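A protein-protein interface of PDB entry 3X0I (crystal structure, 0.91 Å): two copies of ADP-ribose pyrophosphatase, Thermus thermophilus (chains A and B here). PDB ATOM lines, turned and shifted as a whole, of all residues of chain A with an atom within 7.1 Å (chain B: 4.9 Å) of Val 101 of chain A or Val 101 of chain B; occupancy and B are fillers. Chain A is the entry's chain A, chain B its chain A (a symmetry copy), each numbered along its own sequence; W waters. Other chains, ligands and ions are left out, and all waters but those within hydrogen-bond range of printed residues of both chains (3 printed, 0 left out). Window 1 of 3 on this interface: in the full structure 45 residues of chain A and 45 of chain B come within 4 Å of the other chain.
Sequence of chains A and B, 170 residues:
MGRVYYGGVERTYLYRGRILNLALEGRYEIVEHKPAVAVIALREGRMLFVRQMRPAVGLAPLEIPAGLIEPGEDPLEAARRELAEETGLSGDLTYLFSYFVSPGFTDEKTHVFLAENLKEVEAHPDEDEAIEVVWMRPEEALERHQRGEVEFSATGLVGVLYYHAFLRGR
O of Phe 152 of chain A sits at hydrogen-bond distance from N of Phe 100 of chain B. The side-chain hydroxyl of Ser 102 of chain A sits at hydrogen-bond distance from the side-chain carboxylate of Glu 108 of chain B (2.6 Å). The backbone NH (N) of Ala 154 of chain A lies within hydrogen-bond range of the backbone carbonyl oxygen (O) of Phe 100 of chain B (2.8 Å). O of Phe 100 of chain A lies within hydrogen-bond range of N of Ala 154 of chain B. The side-chain hydroxyl (OG) of Ser 102 of chain B lies within hydrogen-bond range of the side-chain carboxylate (OE1) of Glu 108 of chain A (2.6 Å).
Tyr 99 of chain A touches Ala 154 of chain B, and with the chains exchanged Ala 154 of chain A touches Tyr 99 of chain B. Val 101 of chain B touches its own counterpart, Val 101 of chain A. Val 101 of chain A touches Ala 154 of chain B, and with the chains exchanged Ala 154 of chain A touches Val 101 of chain B. Ser 102 of chain A touches Glu 108 of chain B, and with the chains exchanged Glu 108 of chain A touches Ser 102 of chain B. Of the 15 pairs that touch across the chains among the printed residues, 9 have their exchanged pair printed and touching as well.
Of chain B, only Val 101 (3.5 Å) and Ala 154 (3.7 Å) come within 4 Å of Val 101 of chain A. Of chain A, only Val 101 and Ala 154 come within 4 Å of Val 101 of chain B. Printed residues of chain A within 4 Å of Glu 108 of chain B: Ser 102 and Phe 105. Of the printed residues of chain B, Phe 105 of chain A touches Glu 108. Of the printed residues of chain B, Ala 154 of chain A touches Tyr 99, Phe 100 and Val 101. Of the printed residues of chain B, Phe 152 of chain A touches Tyr 99 (3.3 Å) and Phe 100 (2.9 Å). The nearest residue of chain B that does not touch Val 101 of chain A is Ser 102 of chain B (4.1 Å).
Water W3 bridges the backbone carbonyl oxygen of Val 101 of chain A and the side-chain hydroxyl of Tyr 99 of chain B. Water W1 lies within hydrogen-bond range of O of Val 101 of chain B (2.8 Å) and OH of Tyr 99 of chain A (2.8 Å). Water W2 bridges O of Val 101 of chain A (2.9 Å) and O of Val 101 of chain B (2.9 Å).
The backbone NH of Val 101 of chain A is in hydrogen-bond range of the backbone carbonyl oxygen of Glu 108 of chain A (3.1 Å). OG1 of Thr 106 of chain B is in hydrogen-bond range of N of Glu 108 of chain B (3.3 Å). The side-chain hydroxyl (OG) of Ser 153 of chain A sits at hydrogen-bond distance from the side-chain hydroxyl (OG1) of Thr 155 of chain A (2.9 Å). O of Glu 108 of chain B is in hydrogen-bond range of N of Val 101 of chain B (3.1 Å). N of Glu 108 of chain A sits at hydrogen-bond distance from OG1 of Thr 106 of chain A (3.3 Å). The backbone NH (N) of Thr 110 of chain B sits at hydrogen-bond distance from the backbone carbonyl oxygen (O) of Tyr 99 of chain B, 2.8 Å away.
Tyr 99 of chain A touches Ala 154 of chain B. CB of Val 101 of chain A touches O of Val 101 of chain B, at 3.5 Å. Val 101 of chain A touches Ala 154 of chain B. Phe 105 of chain A touches Glu 108 of chain B. O of Phe 152 of chain A touches CA of Tyr 99 of chain B, at 3.3 Å. C of Ser 153 of chain A touches CB of Tyr 99 of chain B, at 3.9 Å. Ser 153 of chain A touches Phe 100 of chain B (CA to O, 3.4 Å). Pro 103 of chain B touches Ser 153 of chain A (CG to CB, 3.8 Å). Ala 154 of chain A touches Tyr 99 of chain B. Val 101 of chain B touches Ala 154 of chain A.
Of the 18 printed residues of chain A, 9 touch a printed residue of chain B. Of the 9 printed residues of chain B, 7 touch a printed residue of chain A. Among the printed residues, 15 pairs touch across the chains. Among the printed residues, no Asp or Glu carboxylate lies within 4 Å of a Lys or Arg side-chain nitrogen of the other chain.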
ATOM      1  N   HIS A  33      16.688  -1.555   4.409  1.00  0.00           N
ATOM      2  CA  HIS A  33      16.635  -0.133   4.293  1.00  0.00           C
ATOM      3  C   HIS A  33      16.273   0.259   2.880  1.00  0.00           C
ATOM      4  O   HIS A  33      16.734  -0.390   1.933  1.00  0.00           O
ATOM      5  CB  HIS A  33      18.039   0.402   4.656  1.00  0.00           C
ATOM      6  CG  HIS A  33      18.202   1.880   4.759  1.00  0.00           C
ATOM      7  ND1 HIS A  33      18.166   2.747   3.685  1.00  0.00           N
ATOM      8  CD2 HIS A  33      18.502   2.652   5.852  1.00  0.00           C
ATOM      9  CE1 HIS A  33      18.435   3.980   4.118  1.00  0.00           C
ATOM     10  NE2 HIS A  33      18.635   3.956   5.434  1.00  0.00           N
ATOM     11  N   ALA A  36      18.797   4.378  -2.000  1.00  0.00           N
ATOM     12  CA  ALA A  36      19.144   5.761  -1.939  1.00  0.00           C
ATOM     13  C   ALA A  36      19.762   6.223  -3.270  1.00  0.00           C
ATOM     14  O   ALA A  36      20.176   5.419  -4.103  1.00  0.00           O
ATOM     15  CB  ALA A  36      20.127   6.021  -0.778  1.00  0.00           C
ATOM     16  N   TYR A  99      26.415   1.313  -5.282  1.00  0.00           N
ATOM     17  CA  TYR A  99      27.140   0.555  -4.294  1.00  0.00           C
ATOM     18  C   TYR A  99      26.227   0.212  -3.115  1.00  0.00           C
ATOM     19  O   TYR A  99      25.330   0.955  -2.766  1.00  0.00           O
ATOM     20  CB  TYR A  99      28.405   1.295  -3.801  1.00  0.00           C
ATOM     21  CG  TYR A  99      28.114   2.557  -3.021  1.00  0.00           C
ATOM     22  CD1 TYR A  99      27.934   3.783  -3.670  1.00  0.00           C
ATOM     23  CD2 TYR A  99      28.003   2.545  -1.648  1.00  0.00           C
ATOM     24  CE1 TYR A  99      27.660   4.927  -2.968  1.00  0.00           C
ATOM     25  CE2 TYR A  99      27.730   3.694  -0.914  1.00  0.00           C
ATOM     26  CZ  TYR A  99      27.541   4.905  -1.574  1.00  0.00           C
ATOM     27  OH  TYR A  99      27.257   6.080  -0.938  1.00  0.00           O
ATOM     28  N   PHE A 100      26.540  -0.915  -2.494  1.00  0.00           N
ATOM     29  CA  PHE A 100      25.946  -1.282  -1.206  1.00  0.00           C
ATOM     30  C   PHE A 100      26.737  -0.654  -0.091  1.00  0.00           C
ATOM     31  O   PHE A 100      27.943  -0.836   0.027  1.00  0.00           O
ATOM     32  CB  PHE A 100      25.948  -2.822  -1.057  1.00  0.00           C
ATOM     33  CG  PHE A 100      24.956  -3.481  -1.981  1.00  0.00           C
ATOM     34  CD1 PHE A 100      25.324  -4.169  -3.069  1.00  0.00           C
ATOM     35  CD2 PHE A 100      23.590  -3.408  -1.691  1.00  0.00           C
ATOM     36  CE1 PHE A 100      24.372  -4.844  -3.870  1.00  0.00           C
ATOM     37  CE2 PHE A 100      22.651  -4.027  -2.493  1.00  0.00           C
ATOM     38  CZ  PHE A 100      23.023  -4.707  -3.599  1.00  0.00           C
ATOM     39  N   VAL A 101      26.045   0.126   0.789  1.00  0.00           N
ATOM     40  CA  VAL A 101      26.750   0.917   1.782  1.00  0.00           C
ATOM     41  C   VAL A 101      27.546   0.071   2.754  1.00  0.00           C
ATOM     42  O   VAL A 101      28.586   0.508   3.222  1.00  0.00           O
ATOM     43  CB  VAL A 101      25.805   1.880   2.566  1.00  0.00           C
ATOM     44  CG1 VAL A 101      24.931   2.667   1.558  1.00  0.00           C
ATOM     45  CG2 VAL A 101      24.948   1.177   3.582  1.00  0.00           C
ATOM     46  N   SER A 102      26.992  -1.104   3.137  1.00  0.00           N
ATOM     47  CA  SER A 102      27.621  -1.958   4.163  1.00  0.00           C
ATOM     48  C   SER A 102      26.967  -3.300   4.075  1.00  0.00           C
ATOM     49  O   SER A 102      26.064  -3.636   4.897  1.00  0.00           O
ATOM     50  CB  SER A 102      27.492  -1.345   5.557  1.00  0.00           C
ATOM     51  OG  SER A 102      28.280  -2.095   6.453  1.00  0.00           O
ATOM     52  N   PRO A 103      27.319  -4.114   3.090  1.00  0.00           N
ATOM     53  CA  PRO A 103      26.548  -5.343   2.800  1.00  0.00           C
ATOM     54  C   PRO A 103      26.750  -6.451   3.867  1.00  0.00           C
ATOM     55  O   PRO A 103      26.056  -7.441   3.784  1.00  0.00           O
ATOM     56  CB  PRO A 103      27.054  -5.757   1.430  1.00  0.00           C
ATOM     57  CG  PRO A 103      28.463  -5.238   1.360  1.00  0.00           C
ATOM     58  CD  PRO A 103      28.421  -3.855   2.104  1.00  0.00           C
ATOM     59  N   GLY A 104      27.663  -6.235   4.835  1.00  0.00           N
ATOM     60  CA  GLY A 104      27.704  -7.128   5.969  1.00  0.00           C
ATOM     61  C   GLY A 104      26.532  -7.060   6.894  1.00  0.00           C
ATOM     62  O   GLY A 104      26.353  -7.944   7.722  1.00  0.00           O
ATOM     63  N   PHE A 105      25.710  -6.005   6.799  1.00  0.00           N
ATOM     64  CA  PHE A 105      24.519  -5.969   7.649  1.00  0.00           C
ATOM     65  C   PHE A 105      23.316  -5.300   7.047  1.00  0.00           C
ATOM     66  O   PHE A 105      22.232  -5.530   7.613  1.00  0.00           O
ATOM     67  CB  PHE A 105      24.823  -5.339   9.033  1.00  0.00           C
ATOM     68  CG  PHE A 105      24.711  -3.822   9.066  1.00  0.00           C
ATOM     69  CD1 PHE A 105      23.560  -3.209   9.589  1.00  0.00           C
ATOM     70  CD2 PHE A 105      25.728  -3.022   8.596  1.00  0.00           C
ATOM     71  CE1 PHE A 105      23.455  -1.857   9.635  1.00  0.00           C
ATOM     72  CE2 PHE A 105      25.604  -1.643   8.660  1.00  0.00           C
ATOM     73  CZ  PHE A 105      24.454  -1.053   9.197  1.00  0.00           C
ATOM     74  N   THR A 106      23.419  -4.499   5.998  1.00  0.00           N
ATOM     75  CA  THR A 106      22.237  -3.827   5.467  1.00  0.00           C
ATOM     76  C   THR A 106      22.177  -4.019   3.967  1.00  0.00           C
ATOM     77  O   THR A 106      23.228  -4.228   3.308  1.00  0.00           O
ATOM     78  CB  THR A 106      22.199  -2.328   5.854  1.00  0.00           C
ATOM     79  OG1 THR A 106      21.020  -1.726   5.345  1.00  0.00           O
ATOM     80  CG2 THR A 106      23.389  -1.540   5.303  1.00  0.00           C
ATOM     81  N   ASP A 107      20.974  -3.928   3.418  1.00  0.00           N
ATOM     82  CA  ASP A 107      20.770  -3.979   1.975  1.00  0.00           C
ATOM     83  C   ASP A 107      20.679  -2.588   1.372  1.00  0.00           C
ATOM     84  O   ASP A 107      20.415  -2.529   0.152  1.00  0.00           O
ATOM     85  CB  ASP A 107      19.544  -4.788   1.573  1.00  0.00           C
ATOM     86  CG  ASP A 107      18.272  -4.193   2.145  1.00  0.00           C
ATOM     87  OD1 ASP A 107      17.252  -4.872   1.901  1.00  0.00           O
ATOM     88  OD2 ASP A 107      18.285  -3.172   2.780  1.00  0.00           O
ATOM     89  N   GLU A 108      20.982  -1.513   2.082  1.00  0.00           N
ATOM     90  CA  GLU A 108      20.896  -0.183   1.479  1.00  0.00           C
ATOM     91  C   GLU A 108      21.854  -0.134   0.247  1.00  0.00           C
ATOM     92  O   GLU A 108      23.049  -0.394   0.387  1.00  0.00           O
ATOM     93  CB  GLU A 108      21.290   0.928   2.458  1.00  0.00           C
ATOM     94  CG  GLU A 108      21.142   2.316   1.824  1.00  0.00           C
ATOM     95  CD  GLU A 108      21.536   3.461   2.737  1.00  0.00           C
ATOM     96  OE1 GLU A 108      21.923   3.211   3.880  1.00  0.00           O
ATOM     97  OE2 GLU A 108      21.425   4.637   2.253  1.00  0.00           O
ATOM     98  N   LYS A 109      21.303   0.255  -0.872  1.00  0.00           N
ATOM     99  CA  LYS A 109      22.011   0.417  -2.118  1.00  0.00           C
ATOM    100  C   LYS A 109      21.860   1.839  -2.602  1.00  0.00           C
ATOM    101  O   LYS A 109      20.750   2.351  -2.622  1.00  0.00           O
ATOM    102  CB  LYS A 109      21.434  -0.542  -3.169  1.00  0.00           C
ATOM    103  CG  LYS A 109      22.287  -0.669  -4.399  1.00  0.00           C
ATOM    104  CD  LYS A 109      21.645  -1.653  -5.398  1.00  0.00           C
ATOM    105  CE  LYS A 109      22.640  -2.008  -6.499  1.00  0.00           C
ATOM    106  NZ  LYS A 109      22.016  -2.881  -7.557  1.00  0.00           N
ATOM    107  N   THR A 110      22.973   2.460  -2.967  1.00  0.00           N
ATOM    108  CA  THR A 110      23.008   3.857  -3.368  1.00  0.00           C
ATOM    109  C   THR A 110      23.341   3.949  -4.837  1.00  0.00           C
ATOM    110  O   THR A 110      24.338   3.391  -5.295  1.00  0.00           O
ATOM    111  CB  THR A 110      24.060   4.596  -2.547  1.00  0.00           C
ATOM    112  OG1 THR A 110      23.789   4.395  -1.170  1.00  0.00           O
ATOM    113  CG2 THR A 110      24.049   6.087  -2.806  1.00  0.00           C
ATOM    114  N   PHE A 152      33.667  12.625   6.404  1.00  0.00           N
ATOM    115  CA  PHE A 152      32.964  12.329   5.168  1.00  0.00           C
ATOM    116  C   PHE A 152      31.874  11.337   5.408  1.00  0.00           C
ATOM    117  O   PHE A 152      32.062  10.386   6.189  1.00  0.00           O
ATOM    118  CB  PHE A 152      33.898  11.679   4.130  1.00  0.00           C
ATOM    119  CG  PHE A 152      34.784  12.631   3.384  1.00  0.00           C
ATOM    120  CD1 PHE A 152      36.148  12.456   3.356  1.00  0.00           C
ATOM    121  CD2 PHE A 152      34.245  13.666   2.614  1.00  0.00           C
ATOM    122  CE1 PHE A 152      36.974  13.284   2.608  1.00  0.00           C
ATOM    123  CE2 PHE A 152      35.034  14.531   1.893  1.00  0.00           C
ATOM    124  CZ  PHE A 152      36.440  14.334   1.889  1.00  0.00           C
ATOM    125  N   SER A 153      30.758  11.461   4.667  1.00  0.00           N
ATOM    126  CA  SER A 153      29.930  10.280   4.425  1.00  0.00           C
ATOM    127  C   SER A 153      30.516   9.502   3.242  1.00  0.00           C
ATOM    128  O   SER A 153      31.341  10.025   2.484  1.00  0.00           O
ATOM    129  CB  SER A 153      28.501  10.674   4.097  1.00  0.00           C
ATOM    130  OG  SER A 153      28.501  11.387   2.851  1.00  0.00           O
ATOM    131  N   ALA A 154      30.026   8.275   3.035  1.00  0.00           N
ATOM    132  CA  ALA A 154      30.408   7.552   1.834  1.00  0.00           C
ATOM    133  C   ALA A 154      30.117   8.376   0.590  1.00  0.00           C
ATOM    134  O   ALA A 154      30.923   8.413  -0.340  1.00  0.00           O
ATOM    135  CB  ALA A 154      29.680   6.216   1.761  1.00  0.00           C
ATOM    136  N   THR A 155      28.952   9.029   0.550  1.00  0.00           N
ATOM    137  CA  THR A 155      28.634   9.780  -0.661  1.00  0.00           C
ATOM    138  C   THR A 155      29.601  10.945  -0.882  1.00  0.00           C
ATOM    139  O   THR A 155      30.002  11.205  -2.025  1.00  0.00           O
ATOM    140  CB  THR A 155      27.160  10.272  -0.672  1.00  0.00           C
ATOM    141  OG1 THR A 155      26.974  11.165   0.441  1.00  0.00           O
ATOM    142  CG2 THR A 155      26.179   9.133  -0.653  1.00  0.00           C
ATOM    143  N   TYR B  99      35.250   7.240   6.323  1.00  0.00           N
ATOM    144  CA  TYR B  99      33.927   7.678   5.954  1.00  0.00           C
ATOM    145  C   TYR B  99      32.876   6.966   6.808  1.00  0.00           C
ATOM    146  O   TYR B  99      33.045   5.833   7.214  1.00  0.00           O
ATOM    147  CB  TYR B  99      33.638   7.461   4.450  1.00  0.00           C
ATOM    148  CG  TYR B  99      33.572   6.007   4.041  1.00  0.00           C
ATOM    149  CD1 TYR B  99      34.728   5.305   3.680  1.00  0.00           C
ATOM    150  CD2 TYR B  99      32.379   5.319   4.017  1.00  0.00           C
ATOM    151  CE1 TYR B  99      34.673   3.984   3.318  1.00  0.00           C
ATOM    152  CE2 TYR B  99      32.300   3.981   3.649  1.00  0.00           C
ATOM    153  CZ  TYR B  99      33.459   3.290   3.304  1.00  0.00           C
ATOM    154  OH  TYR B  99      33.478   1.973   2.942  1.00  0.00           O
ATOM    155  N   PHE B 100      31.771   7.668   7.008  1.00  0.00           N
ATOM    156  CA  PHE B 100      30.565   7.068   7.584  1.00  0.00           C
ATOM    157  C   PHE B 100      29.752   6.429   6.493  1.00  0.00           C
ATOM    158  O   PHE B 100      29.382   7.059   5.509  1.00  0.00           O
ATOM    159  CB  PHE B 100      29.733   8.164   8.294  1.00  0.00           C
ATOM    160  CG  PHE B 100      30.396   8.646   9.559  1.00  0.00           C
ATOM    161  CD1 PHE B 100      30.981   9.846   9.660  1.00  0.00           C
ATOM    162  CD2 PHE B 100      30.383   7.833  10.697  1.00  0.00           C
ATOM    163  CE1 PHE B 100      31.523  10.300  10.886  1.00  0.00           C
ATOM    164  CE2 PHE B 100      30.948   8.251  11.886  1.00  0.00           C
ATOM    165  CZ  PHE B 100      31.553   9.456  11.981  1.00  0.00           C
ATOM    166  N   VAL B 101      29.440   5.110   6.651  1.00  0.00           N
ATOM    167  CA  VAL B 101      28.821   4.365   5.569  1.00  0.00           C
ATOM    168  C   VAL B 101      27.462   4.909   5.180  1.00  0.00           C
ATOM    169  O   VAL B 101      27.091   4.831   4.019  1.00  0.00           O
ATOM    170  CB  VAL B 101      28.716   2.838   5.873  1.00  0.00           C
ATOM    171  CG1 VAL B 101      30.091   2.320   6.361  1.00  0.00           C
ATOM    172  CG2 VAL B 101      27.635   2.501   6.863  1.00  0.00           C
ATOM    173  N   SER B 102      26.676   5.364   6.185  1.00  0.00           N
ATOM    174  CA  SER B 102      25.291   5.813   5.941  1.00  0.00           C
ATOM    175  C   SER B 102      24.858   6.572   7.155  1.00  0.00           C
ATOM    176  O   SER B 102      24.121   6.028   8.030  1.00  0.00           O
ATOM    177  CB  SER B 102      24.366   4.634   5.637  1.00  0.00           C
ATOM    178  OG  SER B 102      23.119   5.138   5.217  1.00  0.00           O
ATOM    179  N   PRO B 103      25.298   7.810   7.320  1.00  0.00           N
ATOM    180  CA  PRO B 103      25.111   8.525   8.601  1.00  0.00           C
ATOM    181  C   PRO B 103      23.641   8.953   8.848  1.00  0.00           C
ATOM    182  O   PRO B 103      23.368   9.424   9.931  1.00  0.00           O
ATOM    183  CB  PRO B 103      26.048   9.713   8.477  1.00  0.00           C
ATOM    184  CG  PRO B 103      26.130   9.995   7.004  1.00  0.00           C
ATOM    185  CD  PRO B 103      26.113   8.581   6.322  1.00  0.00           C
ATOM    186  N   THR B 106      23.166   4.958  10.657  1.00  0.00           N
ATOM    187  CA  THR B 106      24.119   4.163  11.426  1.00  0.00           C
ATOM    188  C   THR B 106      25.356   4.987  11.706  1.00  0.00           C
ATOM    189  O   THR B 106      25.679   5.933  10.942  1.00  0.00           O
ATOM    190  CB  THR B 106      24.466   2.830  10.717  1.00  0.00           C
ATOM    191  OG1 THR B 106      25.366   2.079  11.515  1.00  0.00           O
ATOM    192  CG2 THR B 106      25.127   3.036   9.353  1.00  0.00           C
ATOM    193  N   GLU B 108      28.333   3.437  11.747  1.00  0.00           N
ATOM    194  CA  GLU B 108      29.479   2.676  11.252  1.00  0.00           C
ATOM    195  C   GLU B 108      30.437   3.656  10.500  1.00  0.00           C
ATOM    196  O   GLU B 108      30.013   4.329   9.562  1.00  0.00           O
ATOM    197  CB  GLU B 108      29.066   1.555  10.293  1.00  0.00           C
ATOM    198  CG  GLU B 108      30.276   0.737   9.827  1.00  0.00           C
ATOM    199  CD  GLU B 108      29.936  -0.379   8.859  1.00  0.00           C
ATOM    200  OE1 GLU B 108      28.761  -0.552   8.532  1.00  0.00           O
ATOM    201  OE2 GLU B 108      30.912  -1.091   8.446  1.00  0.00           O
ATOM    202  N   THR B 110      34.266   3.717   8.592  1.00  0.00           N
ATOM    203  CA  THR B 110      35.247   2.865   7.940  1.00  0.00           C
ATOM    204  C   THR B 110      36.528   3.640   7.739  1.00  0.00           C
ATOM    205  O   THR B 110      36.524   4.731   7.169  1.00  0.00           O
ATOM    206  CB  THR B 110      34.703   2.399   6.593  1.00  0.00           C
ATOM    207  OG1 THR B 110      33.444   1.779   6.800  1.00  0.00           O
ATOM    208  CG2 THR B 110      35.610   1.390   5.924  1.00  0.00           C
ATOM    209  N   ALA B 154      30.568  -0.297  -0.885  1.00  0.00           N
ATOM    210  CA  ALA B 154      31.234   0.989  -0.770  1.00  0.00           C
ATOM    211  C   ALA B 154      32.746   0.820  -0.788  1.00  0.00           C
ATOM    212  O   ALA B 154      33.455   1.596  -1.429  1.00  0.00           O
ATOM    213  CB  ALA B 154      30.803   1.702   0.505  1.00  0.00           C
HETATM  214  O   HOH W   1      26.118   5.977   1.663  1.00  0.00           O
HETATM  215  O   HOH W   2      29.015   3.301   2.401  1.00  0.00           O
HETATM  216  O   HOH W   3      31.323   0.309   3.752  1.00  0.00           O
